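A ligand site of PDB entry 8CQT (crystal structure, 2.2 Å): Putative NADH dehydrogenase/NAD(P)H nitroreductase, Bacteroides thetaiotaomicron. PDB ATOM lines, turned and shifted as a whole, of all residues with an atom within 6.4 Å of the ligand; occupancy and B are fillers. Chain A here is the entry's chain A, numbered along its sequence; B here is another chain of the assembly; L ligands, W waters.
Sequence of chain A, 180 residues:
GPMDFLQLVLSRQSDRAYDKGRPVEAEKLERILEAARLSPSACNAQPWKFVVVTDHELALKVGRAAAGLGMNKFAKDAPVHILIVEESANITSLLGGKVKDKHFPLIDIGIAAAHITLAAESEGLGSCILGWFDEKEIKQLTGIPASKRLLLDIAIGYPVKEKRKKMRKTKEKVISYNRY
Water W4 bridges an oxygen (O1) of the ligand and the side-chain amide oxygen of Asn 72.
Water W3 lies within hydrogen-bond range of the guanidinium group (NH1) of Arg 16, the guanidinium group (NH2) of Arg 164 and an oxygen (O6) of the ligand.
NH2 of Arg 168 sits at hydrogen-bond distance from O of Leu 38 of chain B, at 3.0 Å.
ND2 of Asn 72 is in hydrogen-bond range of O of Trp 132 (2.8 Å).
O of Ser 14 lies within hydrogen-bond range of NH2 of Arg 164.
The guanidinium group of Arg 168 lies within hydrogen-bond range of the side-chain amide oxygen of Asn 44 of chain B (3.3 Å).
OE1 of Gln 13 is in hydrogen-bond range of N of Arg 164 (3.1 Å).
The backbone NH (N) of Ala 42 of chain B is in hydrogen-bond range of the side-chain carboxylate (OD1) of Asp 108 of chain B, at 3.1 Å.
The backbone NH of Ala 45 of chain B is in hydrogen-bond range of the side-chain hydroxyl of Ser 41 of chain B (3.4 Å).
O of Met 167 is in hydrogen-bond range of ND2 of Asn 44 of chain B (2.9 Å).
The side-chain hydroxyl (OG) of Ser 14 lies within hydrogen-bond range of an oxygen (O9) of the ligand.
The guanidinium group (NE) of Arg 16 lies within hydrogen-bond range of an oxygen (O1) of the ligand, at 2.6 Å.
The guanidinium group (NH2) of Arg 168 is in salt-bridge range of an oxygen (O8) of the ligand (2.7 Å).
The side-chain sulfur of Cys 128 sits at hydrogen-bond distance from a nitrogen (N1) of the ligand, 3.7 Å away.
An oxygen (O9) of the ligand lies within salt-bridge range of the guanidinium group (NH1) of Arg 12 (2.9 Å).
The guanidinium group of Arg 164 lies within salt-bridge range of an oxygen (O7) of the ligand (3.5 Å).
NZ of Lys 166 lies within salt-bridge range of O8 of the ligand (2.7 Å).
A nitrogen (N3) of the ligand sits at hydrogen-bond distance from the backbone NH (N) of Gly 131 (3.0 Å).
N2 of the ligand sits at hydrogen-bond distance from OD1 of Asn 72 (2.8 Å).
The backbone NH (N) of Ser 14 is in hydrogen-bond range of an oxygen (O7) of the ligand.
A nitrogen (N4) of the ligand lies close to the backbone carbonyl oxygen (O) of Ile 129 (3.0 Å).
Gln 13 touches the ligand.
CE of Met 71 touches N2 of the ligand, at 3.9 Å.
Phe 74 touches the ligand.
Leu 130 touches the ligand (CA to O2, 3.6 Å).
Trp 132 touches the ligand (N to O2, 3.5 Å).
Leu 152 touches the ligand (CD2 to C7, 3.9 Å).
CB of Pro 40 of chain B touches O4 of the ligand, 3.2 Å away.
Ser 41 of chain B touches the ligand.
Ala 42 of chain B touches the ligand.
Asn 44 of chain B touches the ligand (OD1 to C17, 3.6 Å).
Phe 104 of chain B touches the ligand (CD1 to C7, 3.9 Å).
Ile 107 of chain B touches the ligand (CG2 to C7, 3.99 Å).
OD1 of Asp 108 of chain B touches C9 of the ligand, at 3.9 Å.
Ile 111 of chain B touches the ligand.
Hydrophobic or aromatic side chains that line the ligand: Met 71, Phe 74, Ile 129, Leu 130, Trp 132, Leu 152, Pro 40 of chain B, Ala 42 of chain B, Phe 104 of chain B, Ile 107 of chain B and Ile 111 of chain B.
The nearest printed residue that does not touch the ligand is Cys 43 of chain B (4.2 Å).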
ATOM      1  N   ARG A  12      22.656  10.120  -9.575  1.00  0.00           N
ATOM      2  CA  ARG A  12      21.844   8.963  -9.217  1.00  0.00           C
ATOM      3  C   ARG A  12      22.096   8.617  -7.759  1.00  0.00           C
ATOM      4  O   ARG A  12      23.243   8.471  -7.365  1.00  0.00           O
ATOM      5  CB  ARG A  12      22.161   7.761 -10.089  1.00  0.00           C
ATOM      6  CG  ARG A  12      21.126   6.653  -9.937  1.00  0.00           C
ATOM      7  CD  ARG A  12      21.443   5.380  -9.177  1.00  0.00           C
ATOM      8  NE  ARG A  12      22.699   5.299  -8.484  1.00  0.00           N
ATOM      9  CZ  ARG A  12      22.777   5.157  -7.168  1.00  0.00           C
ATOM     10  NH1 ARG A  12      21.689   4.888  -6.465  1.00  0.00           N
ATOM     11  NH2 ARG A  12      23.948   5.320  -6.573  1.00  0.00           N
ATOM     12  N   GLN A  13      21.031   8.521  -6.965  1.00  0.00           N
ATOM     13  CA  GLN A  13      21.106   8.171  -5.553  1.00  0.00           C
ATOM     14  C   GLN A  13      19.870   7.356  -5.160  1.00  0.00           C
ATOM     15  O   GLN A  13      18.917   7.240  -5.923  1.00  0.00           O
ATOM     16  CB  GLN A  13      21.214   9.445  -4.692  1.00  0.00           C
ATOM     17  CG  GLN A  13      19.917  10.265  -4.715  1.00  0.00           C
ATOM     18  CD  GLN A  13      19.981  11.366  -3.673  1.00  0.00           C
ATOM     19  OE1 GLN A  13      21.068  11.753  -3.246  1.00  0.00           O
ATOM     20  NE2 GLN A  13      18.821  11.837  -3.210  1.00  0.00           N
ATOM     21  N   SER A  14      19.906   6.807  -3.926  1.00  0.00           N
ATOM     22  CA  SER A  14      18.753   6.097  -3.398  1.00  0.00           C
ATOM     23  C   SER A  14      17.802   7.149  -2.837  1.00  0.00           C
ATOM     24  O   SER A  14      18.018   7.770  -1.759  1.00  0.00           O
ATOM     25  CB  SER A  14      19.164   5.071  -2.398  1.00  0.00           C
ATOM     26  OG  SER A  14      20.060   4.090  -2.915  1.00  0.00           O
ATOM     27  N   ASP A  15      16.707   7.343  -3.572  1.00  0.00           N
ATOM     28  CA  ASP A  15      15.671   8.270  -3.156  1.00  0.00           C
ATOM     29  C   ASP A  15      14.743   7.515  -2.211  1.00  0.00           C
ATOM     30  O   ASP A  15      14.145   6.547  -2.679  1.00  0.00           O
ATOM     31  CB  ASP A  15      14.942   8.881  -4.357  1.00  0.00           C
ATOM     32  CG  ASP A  15      15.890   9.687  -5.227  1.00  0.00           C
ATOM     33  OD1 ASP A  15      16.318  10.735  -4.703  1.00  0.00           O
ATOM     34  OD2 ASP A  15      16.248   9.220  -6.376  1.00  0.00           O
ATOM     35  N   ARG A  16      14.550   8.055  -0.995  1.00  0.00           N
ATOM     36  CA  ARG A  16      13.744   7.430   0.069  1.00  0.00           C
ATOM     37  C   ARG A  16      12.576   8.372   0.427  1.00  0.00           C
ATOM     38  O   ARG A  16      12.103   8.382   1.544  1.00  0.00           O
ATOM     39  CB  ARG A  16      14.629   7.117   1.301  1.00  0.00           C
ATOM     40  CG  ARG A  16      15.717   6.110   0.947  1.00  0.00           C
ATOM     41  CD  ARG A  16      16.432   5.506   2.156  1.00  0.00           C
ATOM     42  NE  ARG A  16      17.419   4.536   1.764  1.00  0.00           N
ATOM     43  CZ  ARG A  16      18.694   4.783   1.389  1.00  0.00           C
ATOM     44  NH1 ARG A  16      19.241   6.011   1.412  1.00  0.00           N
ATOM     45  NH2 ARG A  16      19.431   3.763   1.012  1.00  0.00           N
ATOM     46  N   ALA A  66       7.022  -4.166   1.060  1.00  0.00           N
ATOM     47  CA  ALA A  66       8.451  -3.961   1.116  1.00  0.00           C
ATOM     48  C   ALA A  66       8.922  -3.353   2.447  1.00  0.00           C
ATOM     49  O   ALA A  66      10.098  -3.279   2.671  1.00  0.00           O
ATOM     50  CB  ALA A  66       8.857  -3.104  -0.071  1.00  0.00           C
ATOM     51  N   MET A  71      12.328  -0.258   8.141  1.00  0.00           N
ATOM     52  CA  MET A  71      12.944   0.048   6.856  1.00  0.00           C
ATOM     53  C   MET A  71      11.853   0.254   5.788  1.00  0.00           C
ATOM     54  O   MET A  71      10.734  -0.302   5.909  1.00  0.00           O
ATOM     55  CB  MET A  71      13.833  -1.122   6.390  1.00  0.00           C
ATOM     56  CG  MET A  71      15.204  -1.292   7.101  1.00  0.00           C
ATOM     57  SD  MET A  71      16.261  -2.486   6.113  1.00  0.00           S
ATOM     58  CE  MET A  71      17.229  -1.363   5.113  1.00  0.00           C
ATOM     59  N   ASN A  72      12.194   0.969   4.710  1.00  0.00           N
ATOM     60  CA  ASN A  72      11.438   0.933   3.448  1.00  0.00           C
ATOM     61  C   ASN A  72      10.019   1.476   3.583  1.00  0.00           C
ATOM     62  O   ASN A  72       9.184   1.168   2.733  1.00  0.00           O
ATOM     63  CB  ASN A  72      11.466  -0.483   2.866  1.00  0.00           C
ATOM     64  CG  ASN A  72      12.875  -0.898   2.464  1.00  0.00           C
ATOM     65  OD1 ASN A  72      13.781  -0.053   2.509  1.00  0.00           O
ATOM     66  ND2 ASN A  72      13.105  -2.158   2.120  1.00  0.00           N
ATOM     67  N   PHE A  74       8.996   4.378   2.910  1.00  0.00           N
ATOM     68  CA  PHE A  74       8.738   5.244   1.771  1.00  0.00           C
ATOM     69  C   PHE A  74       8.289   4.417   0.551  1.00  0.00           C
ATOM     70  O   PHE A  74       7.839   5.025  -0.414  1.00  0.00           O
ATOM     71  CB  PHE A  74      10.017   6.037   1.488  1.00  0.00           C
ATOM     72  CG  PHE A  74      11.177   5.130   1.101  1.00  0.00           C
ATOM     73  CD1 PHE A  74      11.318   4.662  -0.194  1.00  0.00           C
ATOM     74  CD2 PHE A  74      12.080   4.689   2.061  1.00  0.00           C
ATOM     75  CE1 PHE A  74      12.328   3.763  -0.534  1.00  0.00           C
ATOM     76  CE2 PHE A  74      13.090   3.795   1.731  1.00  0.00           C
ATOM     77  CZ  PHE A  74      13.179   3.311   0.435  1.00  0.00           C
ATOM     78  N   CYS A 128      15.035   3.677  -6.006  1.00  0.00           N
ATOM     79  CA  CYS A 128      15.720   3.039  -4.902  1.00  0.00           C
ATOM     80  C   CYS A 128      15.634   1.551  -5.115  1.00  0.00           C
ATOM     81  O   CYS A 128      14.545   0.972  -5.153  1.00  0.00           O
ATOM     82  CB  CYS A 128      15.110   3.390  -3.525  1.00  0.00           C
ATOM     83  SG  CYS A 128      16.203   2.957  -2.151  1.00  0.00           S
ATOM     84  N   ILE A 129      16.823   0.910  -5.167  1.00  0.00           N
ATOM     85  CA  ILE A 129      16.915  -0.539  -5.173  1.00  0.00           C
ATOM     86  C   ILE A 129      16.603  -1.047  -3.764  1.00  0.00           C
ATOM     87  O   ILE A 129      17.225  -0.560  -2.805  1.00  0.00           O
ATOM     88  CB  ILE A 129      18.339  -0.956  -5.575  1.00  0.00           C
ATOM     89  CG1 ILE A 129      18.647  -0.488  -6.997  1.00  0.00           C
ATOM     90  CG2 ILE A 129      18.518  -2.459  -5.377  1.00  0.00           C
ATOM     91  CD1 ILE A 129      20.135  -0.496  -7.352  1.00  0.00           C
ATOM     92  N   LEU A 130      15.699  -2.047  -3.673  1.00  0.00           N
ATOM     93  CA  LEU A 130      15.336  -2.678  -2.379  1.00  0.00           C
ATOM     94  C   LEU A 130      15.668  -4.168  -2.453  1.00  0.00           C
ATOM     95  O   LEU A 130      15.134  -4.870  -3.318  1.00  0.00           O
ATOM     96  CB  LEU A 130      13.842  -2.468  -2.026  1.00  0.00           C
ATOM     97  CG  LEU A 130      13.351  -1.040  -2.182  1.00  0.00           C
ATOM     98  CD1 LEU A 130      11.829  -0.938  -1.953  1.00  0.00           C
ATOM     99  CD2 LEU A 130      14.089  -0.145  -1.269  1.00  0.00           C
ATOM    100  N   GLY A 131      16.574  -4.604  -1.574  1.00  0.00           N
ATOM    101  CA  GLY A 131      16.934  -5.993  -1.398  1.00  0.00           C
ATOM    102  C   GLY A 131      16.198  -6.715  -0.254  1.00  0.00           C
ATOM    103  O   GLY A 131      16.212  -7.945  -0.154  1.00  0.00           O
ATOM    104  N   TRP A 132      15.571  -5.893   0.568  1.00  0.00           N
ATOM    105  CA  TRP A 132      14.820  -6.265   1.747  1.00  0.00           C
ATOM    106  C   TRP A 132      13.352  -5.929   1.529  1.00  0.00           C
ATOM    107  O   TRP A 132      12.991  -4.777   1.205  1.00  0.00           O
ATOM    108  CB  TRP A 132      15.330  -5.502   2.987  1.00  0.00           C
ATOM    109  CG  TRP A 132      16.524  -6.183   3.573  1.00  0.00           C
ATOM    110  CD1 TRP A 132      16.571  -7.293   4.363  1.00  0.00           C
ATOM    111  CD2 TRP A 132      17.872  -5.735   3.407  1.00  0.00           C
ATOM    112  NE1 TRP A 132      17.869  -7.593   4.694  1.00  0.00           N
ATOM    113  CE2 TRP A 132      18.684  -6.662   4.114  1.00  0.00           C
ATOM    114  CE3 TRP A 132      18.435  -4.686   2.700  1.00  0.00           C
ATOM    115  CZ2 TRP A 132      20.062  -6.510   4.177  1.00  0.00           C
ATOM    116  CZ3 TRP A 132      19.812  -4.552   2.726  1.00  0.00           C
ATOM    117  CH2 TRP A 132      20.599  -5.450   3.453  1.00  0.00           C
ATOM    118  N   PHE A 133      12.561  -6.979   1.697  1.00  0.00           N
ATOM    119  CA  PHE A 133      11.134  -6.910   1.457  1.00  0.00           C
ATOM    120  C   PHE A 133      10.558  -8.253   1.888  1.00  0.00           C
ATOM    121  O   PHE A 133      11.274  -9.174   2.191  1.00  0.00           O
ATOM    122  CB  PHE A 133      10.819  -6.554  -0.015  1.00  0.00           C
ATOM    123  CG  PHE A 133      11.610  -7.362  -1.009  1.00  0.00           C
ATOM    124  CD1 PHE A 133      11.199  -8.653  -1.342  1.00  0.00           C
ATOM    125  CD2 PHE A 133      12.748  -6.827  -1.615  1.00  0.00           C
ATOM    126  CE1 PHE A 133      11.997  -9.424  -2.153  1.00  0.00           C
ATOM    127  CE2 PHE A 133      13.465  -7.581  -2.509  1.00  0.00           C
ATOM    128  CZ  PHE A 133      13.134  -8.887  -2.726  1.00  0.00           C
ATOM    129  N   LEU A 152      15.003  -8.357  -6.239  1.00  0.00           N
ATOM    130  CA  LEU A 152      15.041  -6.940  -5.976  1.00  0.00           C
ATOM    131  C   LEU A 152      13.686  -6.349  -6.352  1.00  0.00           C
ATOM    132  O   LEU A 152      13.015  -6.822  -7.282  1.00  0.00           O
ATOM    133  CB  LEU A 152      16.148  -6.325  -6.857  1.00  0.00           C
ATOM    134  CG  LEU A 152      17.607  -6.701  -6.562  1.00  0.00           C
ATOM    135  CD1 LEU A 152      18.514  -6.004  -7.533  1.00  0.00           C
ATOM    136  CD2 LEU A 152      18.043  -6.327  -5.166  1.00  0.00           C
ATOM    137  N   ARG A 164      21.656  14.249  -1.525  1.00  0.00           N
ATOM    138  CA  ARG A 164      22.618  14.085  -0.461  1.00  0.00           C
ATOM    139  C   ARG A 164      24.011  13.870  -1.055  1.00  0.00           C
ATOM    140  O   ARG A 164      24.174  13.387  -2.187  1.00  0.00           O
ATOM    141  CB  ARG A 164      22.247  12.860   0.383  1.00  0.00           C
ATOM    142  CG  ARG A 164      20.852  12.917   0.968  1.00  0.00           C
ATOM    143  CD  ARG A 164      20.448  11.646   1.714  1.00  0.00           C
ATOM    144  NE  ARG A 164      20.740  10.402   1.000  1.00  0.00           N
ATOM    145  CZ  ARG A 164      19.910   9.776   0.143  1.00  0.00           C
ATOM    146  NH1 ARG A 164      18.676  10.202  -0.031  1.00  0.00           N
ATOM    147  NH2 ARG A 164      20.317   8.700  -0.506  1.00  0.00           N
ATOM    148  N   LYS A 166      27.457  11.863  -1.410  1.00  0.00           N
ATOM    149  CA  LYS A 166      27.837  10.473  -1.447  1.00  0.00           C
ATOM    150  C   LYS A 166      28.844  10.135  -0.365  1.00  0.00           C
ATOM    151  O   LYS A 166      29.805  10.891  -0.165  1.00  0.00           O
ATOM    152  CB  LYS A 166      28.566  10.113  -2.757  1.00  0.00           C
ATOM    153  CG  LYS A 166      27.755  10.188  -4.040  1.00  0.00           C
ATOM    154  CD  LYS A 166      26.730   9.105  -4.115  1.00  0.00           C
ATOM    155  CE  LYS A 166      25.783   9.355  -5.256  1.00  0.00           C
ATOM    156  NZ  LYS A 166      24.569   8.542  -5.101  1.00  0.00           N
ATOM    157  N   MET A 167      28.674   8.973   0.259  1.00  0.00           N
ATOM    158  CA  MET A 167      29.730   8.416   1.058  1.00  0.00           C
ATOM    159  C   MET A 167      30.186   7.123   0.361  1.00  0.00           C
ATOM    160  O   MET A 167      29.387   6.201   0.171  1.00  0.00           O
ATOM    161  CB  MET A 167      29.240   8.172   2.486  1.00  0.00           C
ATOM    162  CG  MET A 167      29.233   9.480   3.302  1.00  0.00           C
ATOM    163  SD  MET A 167      28.199   9.387   4.778  1.00  0.00           S
ATOM    164  CE  MET A 167      26.635   8.771   4.152  1.00  0.00           C
ATOM    165  N   ARG A 168      31.488   7.081   0.088  1.00  0.00           N
ATOM    166  CA  ARG A 168      32.181   5.928  -0.467  1.00  0.00           C
ATOM    167  C   ARG A 168      33.501   5.760   0.279  1.00  0.00           C
ATOM    168  O   ARG A 168      34.027   6.725   0.751  1.00  0.00           O
ATOM    169  CB  ARG A 168      32.376   6.091  -1.986  1.00  0.00           C
ATOM    170  CG  ARG A 168      31.083   5.983  -2.806  1.00  0.00           C
ATOM    171  CD  ARG A 168      30.232   4.708  -2.655  1.00  0.00           C
ATOM    172  NE  ARG A 168      29.069   4.700  -3.554  1.00  0.00           N
ATOM    173  CZ  ARG A 168      27.892   5.265  -3.273  1.00  0.00           C
ATOM    174  NH1 ARG A 168      27.654   5.829  -2.100  1.00  0.00           N
ATOM    175  NH2 ARG A 168      26.910   5.271  -4.164  1.00  0.00           N
ATOM    176  N   LEU B  38      31.752   4.851  -7.192  1.00  0.00           N
ATOM    177  CA  LEU B  38      30.497   5.521  -6.904  1.00  0.00           C
ATOM    178  C   LEU B  38      29.286   4.610  -7.137  1.00  0.00           C
ATOM    179  O   LEU B  38      28.180   5.065  -6.892  1.00  0.00           O
ATOM    180  CB  LEU B  38      30.337   6.715  -7.844  1.00  0.00           C
ATOM    181  CG  LEU B  38      31.281   7.907  -7.630  1.00  0.00           C
ATOM    182  CD1 LEU B  38      30.976   9.019  -8.635  1.00  0.00           C
ATOM    183  CD2 LEU B  38      31.184   8.497  -6.242  1.00  0.00           C
ATOM    184  N   SER B  39      29.469   3.361  -7.552  1.00  0.00           N
ATOM    185  CA  SER B  39      28.331   2.429  -7.665  1.00  0.00           C
ATOM    186  C   SER B  39      27.555   2.306  -6.354  1.00  0.00           C
ATOM    187  O   SER B  39      28.156   2.329  -5.257  1.00  0.00           O
ATOM    188  CB  SER B  39      28.809   1.056  -8.042  1.00  0.00           C
ATOM    189  OG  SER B  39      29.467   1.055  -9.318  1.00  0.00           O
ATOM    190  N   PRO B  40      26.214   2.118  -6.411  1.00  0.00           N
ATOM    191  CA  PRO B  40      25.473   1.715  -5.227  1.00  0.00           C
ATOM    192  C   PRO B  40      25.783   0.270  -4.817  1.00  0.00           C
ATOM    193  O   PRO B  40      26.177  -0.539  -5.669  1.00  0.00           O
ATOM    194  CB  PRO B  40      23.984   1.866  -5.653  1.00  0.00           C
ATOM    195  CG  PRO B  40      24.019   1.564  -7.141  1.00  0.00           C
ATOM    196  CD  PRO B  40      25.334   2.224  -7.594  1.00  0.00           C
ATOM    197  N   SER B  41      25.453  -0.085  -3.553  1.00  0.00           N
ATOM    198  CA  SER B  41      25.601  -1.437  -3.015  1.00  0.00           C
ATOM    199  C   SER B  41      24.685  -1.605  -1.787  1.00  0.00           C
ATOM    200  O   SER B  41      24.484  -0.623  -1.054  1.00  0.00           O
ATOM    201  CB  SER B  41      27.087  -1.720  -2.657  1.00  0.00           C
ATOM    202  OG  SER B  41      27.587  -0.749  -1.748  1.00  0.00           O
ATOM    203  N   ALA B  42      24.138  -2.826  -1.531  1.00  0.00           N
ATOM    204  CA  ALA B  42      23.327  -3.012  -0.321  1.00  0.00           C
ATOM    205  C   ALA B  42      24.138  -2.547   0.900  1.00  0.00           C
ATOM    206  O   ALA B  42      25.327  -2.865   0.975  1.00  0.00           O
ATOM    207  CB  ALA B  42      22.844  -4.449  -0.138  1.00  0.00           C
ATOM    208  N   CYS B  43      23.493  -1.746   1.767  1.00  0.00           N
ATOM    209  CA  CYS B  43      24.056  -1.260   3.033  1.00  0.00           C
ATOM    210  C   CYS B  43      25.246  -0.339   2.767  1.00  0.00           C
ATOM    211  O   CYS B  43      26.034  -0.044   3.671  1.00  0.00           O
ATOM    212  CB  CYS B  43      24.507  -2.416   3.952  1.00  0.00           C
ATOM    213  SG  CYS B  43      23.156  -3.507   4.492  1.00  0.00           S
ATOM    214  N   ASN B  44      25.473   0.049   1.491  1.00  0.00           N
ATOM    215  CA  ASN B  44      26.670   0.807   1.162  1.00  0.00           C
ATOM    216  C   ASN B  44      27.930   0.059   1.577  1.00  0.00           C
ATOM    217  O   ASN B  44      28.970   0.680   1.820  1.00  0.00           O
ATOM    218  CB  ASN B  44      26.730   2.201   1.807  1.00  0.00           C
ATOM    219  CG  ASN B  44      27.573   3.195   1.048  1.00  0.00           C
ATOM    220  OD1 ASN B  44      27.769   3.117  -0.191  1.00  0.00           O
ATOM    221  ND2 ASN B  44      28.111   4.157   1.813  1.00  0.00           N
ATOM    222  N   ALA B  45      27.871  -1.296   1.598  1.00  0.00           N
ATOM    223  CA  ALA B  45      29.016  -2.098   2.013  1.00  0.00           C
ATOM    224  C   ALA B  45      30.171  -2.072   1.003  1.00  0.00           C
ATOM    225  O   ALA B  45      31.335  -2.298   1.403  1.00  0.00           O
ATOM    226  CB  ALA B  45      28.582  -3.519   2.320  1.00  0.00           C
ATOM    227  N   PHE B 104      24.298 -10.446  -1.848  1.00  0.00           N
ATOM    228  CA  PHE B 104      24.365  -9.049  -2.205  1.00  0.00           C
ATOM    229  C   PHE B 104      25.710  -8.715  -2.841  1.00  0.00           C
ATOM    230  O   PHE B 104      25.713  -8.048  -3.834  1.00  0.00           O
ATOM    231  CB  PHE B 104      24.041  -8.183  -1.004  1.00  0.00           C
ATOM    232  CG  PHE B 104      22.563  -8.112  -0.681  1.00  0.00           C
ATOM    233  CD1 PHE B 104      21.598  -8.111  -1.672  1.00  0.00           C
ATOM    234  CD2 PHE B 104      22.153  -7.968   0.635  1.00  0.00           C
ATOM    235  CE1 PHE B 104      20.256  -8.040  -1.356  1.00  0.00           C
ATOM    236  CE2 PHE B 104      20.796  -7.859   0.944  1.00  0.00           C
ATOM    237  CZ  PHE B 104      19.856  -7.879  -0.049  1.00  0.00           C
ATOM    238  N   ILE B 107      25.433  -9.229  -6.511  1.00  0.00           N
ATOM    239  CA  ILE B 107      24.571  -8.240  -7.146  1.00  0.00           C
ATOM    240  C   ILE B 107      25.381  -6.944  -7.238  1.00  0.00           C
ATOM    241  O   ILE B 107      25.459  -6.304  -8.276  1.00  0.00           O
ATOM    242  CB  ILE B 107      23.236  -8.125  -6.369  1.00  0.00           C
ATOM    243  CG1 ILE B 107      22.365  -9.361  -6.598  1.00  0.00           C
ATOM    244  CG2 ILE B 107      22.472  -6.900  -6.736  1.00  0.00           C
ATOM    245  CD1 ILE B 107      21.161  -9.500  -5.652  1.00  0.00           C
ATOM    246  N   ASP B 108      26.092  -6.609  -6.171  1.00  0.00           N
ATOM    247  CA  ASP B 108      26.825  -5.366  -6.064  1.00  0.00           C
ATOM    248  C   ASP B 108      27.893  -5.301  -7.134  1.00  0.00           C
ATOM    249  O   ASP B 108      28.111  -4.252  -7.759  1.00  0.00           O
ATOM    250  CB  ASP B 108      27.488  -5.257  -4.689  1.00  0.00           C
ATOM    251  CG  ASP B 108      26.596  -5.103  -3.468  1.00  0.00           C
ATOM    252  OD1 ASP B 108      25.392  -4.806  -3.588  1.00  0.00           O
ATOM    253  OD2 ASP B 108      27.155  -5.331  -2.388  1.00  0.00           O
ATOM    254  N   ILE B 111      26.424  -4.505 -10.532  1.00  0.00           N
ATOM    255  CA  ILE B 111      26.253  -3.056 -10.534  1.00  0.00           C
ATOM    256  C   ILE B 111      27.545  -2.353 -10.940  1.00  0.00           C
ATOM    257  O   ILE B 111      27.575  -1.470 -11.820  1.00  0.00           O
ATOM    258  CB  ILE B 111      25.731  -2.548  -9.185  1.00  0.00           C
ATOM    259  CG1 ILE B 111      24.331  -3.088  -8.947  1.00  0.00           C
ATOM    260  CG2 ILE B 111      25.751  -1.007  -9.154  1.00  0.00           C
ATOM    261  CD1 ILE B 111      23.760  -2.808  -7.525  1.00  0.00           C
HETATM  262  N1  LIG L   1      18.092   1.083   0.396  1.00  0.00           N
HETATM  263  C1  LIG L   1      17.017   1.029   1.237  1.00  0.00           C
HETATM  264  O1  LIG L   1      16.594   2.029   1.812  1.00  0.00           O
HETATM  265  N2  LIG L   1      16.412  -0.202   1.455  1.00  0.00           N
HETATM  266  C2  LIG L   1      16.763  -1.407   0.897  1.00  0.00           C
HETATM  267  O2  LIG L   1      16.109  -2.440   1.095  1.00  0.00           O
HETATM  268  C3  LIG L   1      17.909  -1.345   0.094  1.00  0.00           C
HETATM  269  N3  LIG L   1      18.351  -2.457  -0.459  1.00  0.00           N
HETATM  270  C4  LIG L   1      19.343  -2.349  -1.390  1.00  0.00           C
HETATM  271  C5  LIG L   1      19.789  -3.502  -2.035  1.00  0.00           C
HETATM  272  C6  LIG L   1      20.845  -3.488  -2.899  1.00  0.00           C
HETATM  273  C7  LIG L   1      21.289  -4.759  -3.585  1.00  0.00           C
HETATM  274  C8  LIG L   1      21.433  -2.293  -3.222  1.00  0.00           C
HETATM  275  C9  LIG L   1      22.519  -2.240  -4.231  1.00  0.00           C
HETATM  276  C10 LIG L   1      21.034  -1.118  -2.613  1.00  0.00           C
HETATM  277  C11 LIG L   1      20.034  -1.168  -1.632  1.00  0.00           C
HETATM  278  N4  LIG L   1      19.573  -0.027  -1.014  1.00  0.00           N
HETATM  279  C12 LIG L   1      18.487  -0.053  -0.154  1.00  0.00           C
HETATM  280  C13 LIG L   1      20.228   1.236  -1.341  1.00  0.00           C
HETATM  281  C14 LIG L   1      21.629   1.356  -0.745  1.00  0.00           C
HETATM  282  O3  LIG L   1      21.461   1.703   0.635  1.00  0.00           O
HETATM  283  C15 LIG L   1      22.377   2.499  -1.431  1.00  0.00           C
HETATM  284  O4  LIG L   1      22.543   2.192  -2.810  1.00  0.00           O
HETATM  285  C16 LIG L   1      23.728   2.837  -0.754  1.00  0.00           C
HETATM  286  O5  LIG L   1      23.537   3.272   0.617  1.00  0.00           O
HETATM  287  C17 LIG L   1      24.551   3.894  -1.489  1.00  0.00           C
HETATM  288  O6  LIG L   1      23.756   5.070  -1.526  1.00  0.00           O
HETATM  289  P1  LIG L   1      23.258   5.702  -2.972  1.00  0.00           P
HETATM  290  O7  LIG L   1      22.429   6.835  -2.514  1.00  0.00           O
HETATM  291  O8  LIG L   1      24.457   6.192  -3.726  1.00  0.00           O
HETATM  292  O9  LIG L   1      22.473   4.518  -3.681  1.00  0.00           O
HETATM  293  O   HOH W   1      23.882   8.862  -1.401  1.00  0.00           O
HETATM  294  O   HOH W   2      24.679   5.672   1.486  1.00  0.00           O
HETATM  295  O   HOH W   3      21.753   6.274   0.591  1.00  0.00           O
HETATM  296  O   HOH W   4      15.380   2.013   4.236  1.00  0.00           O
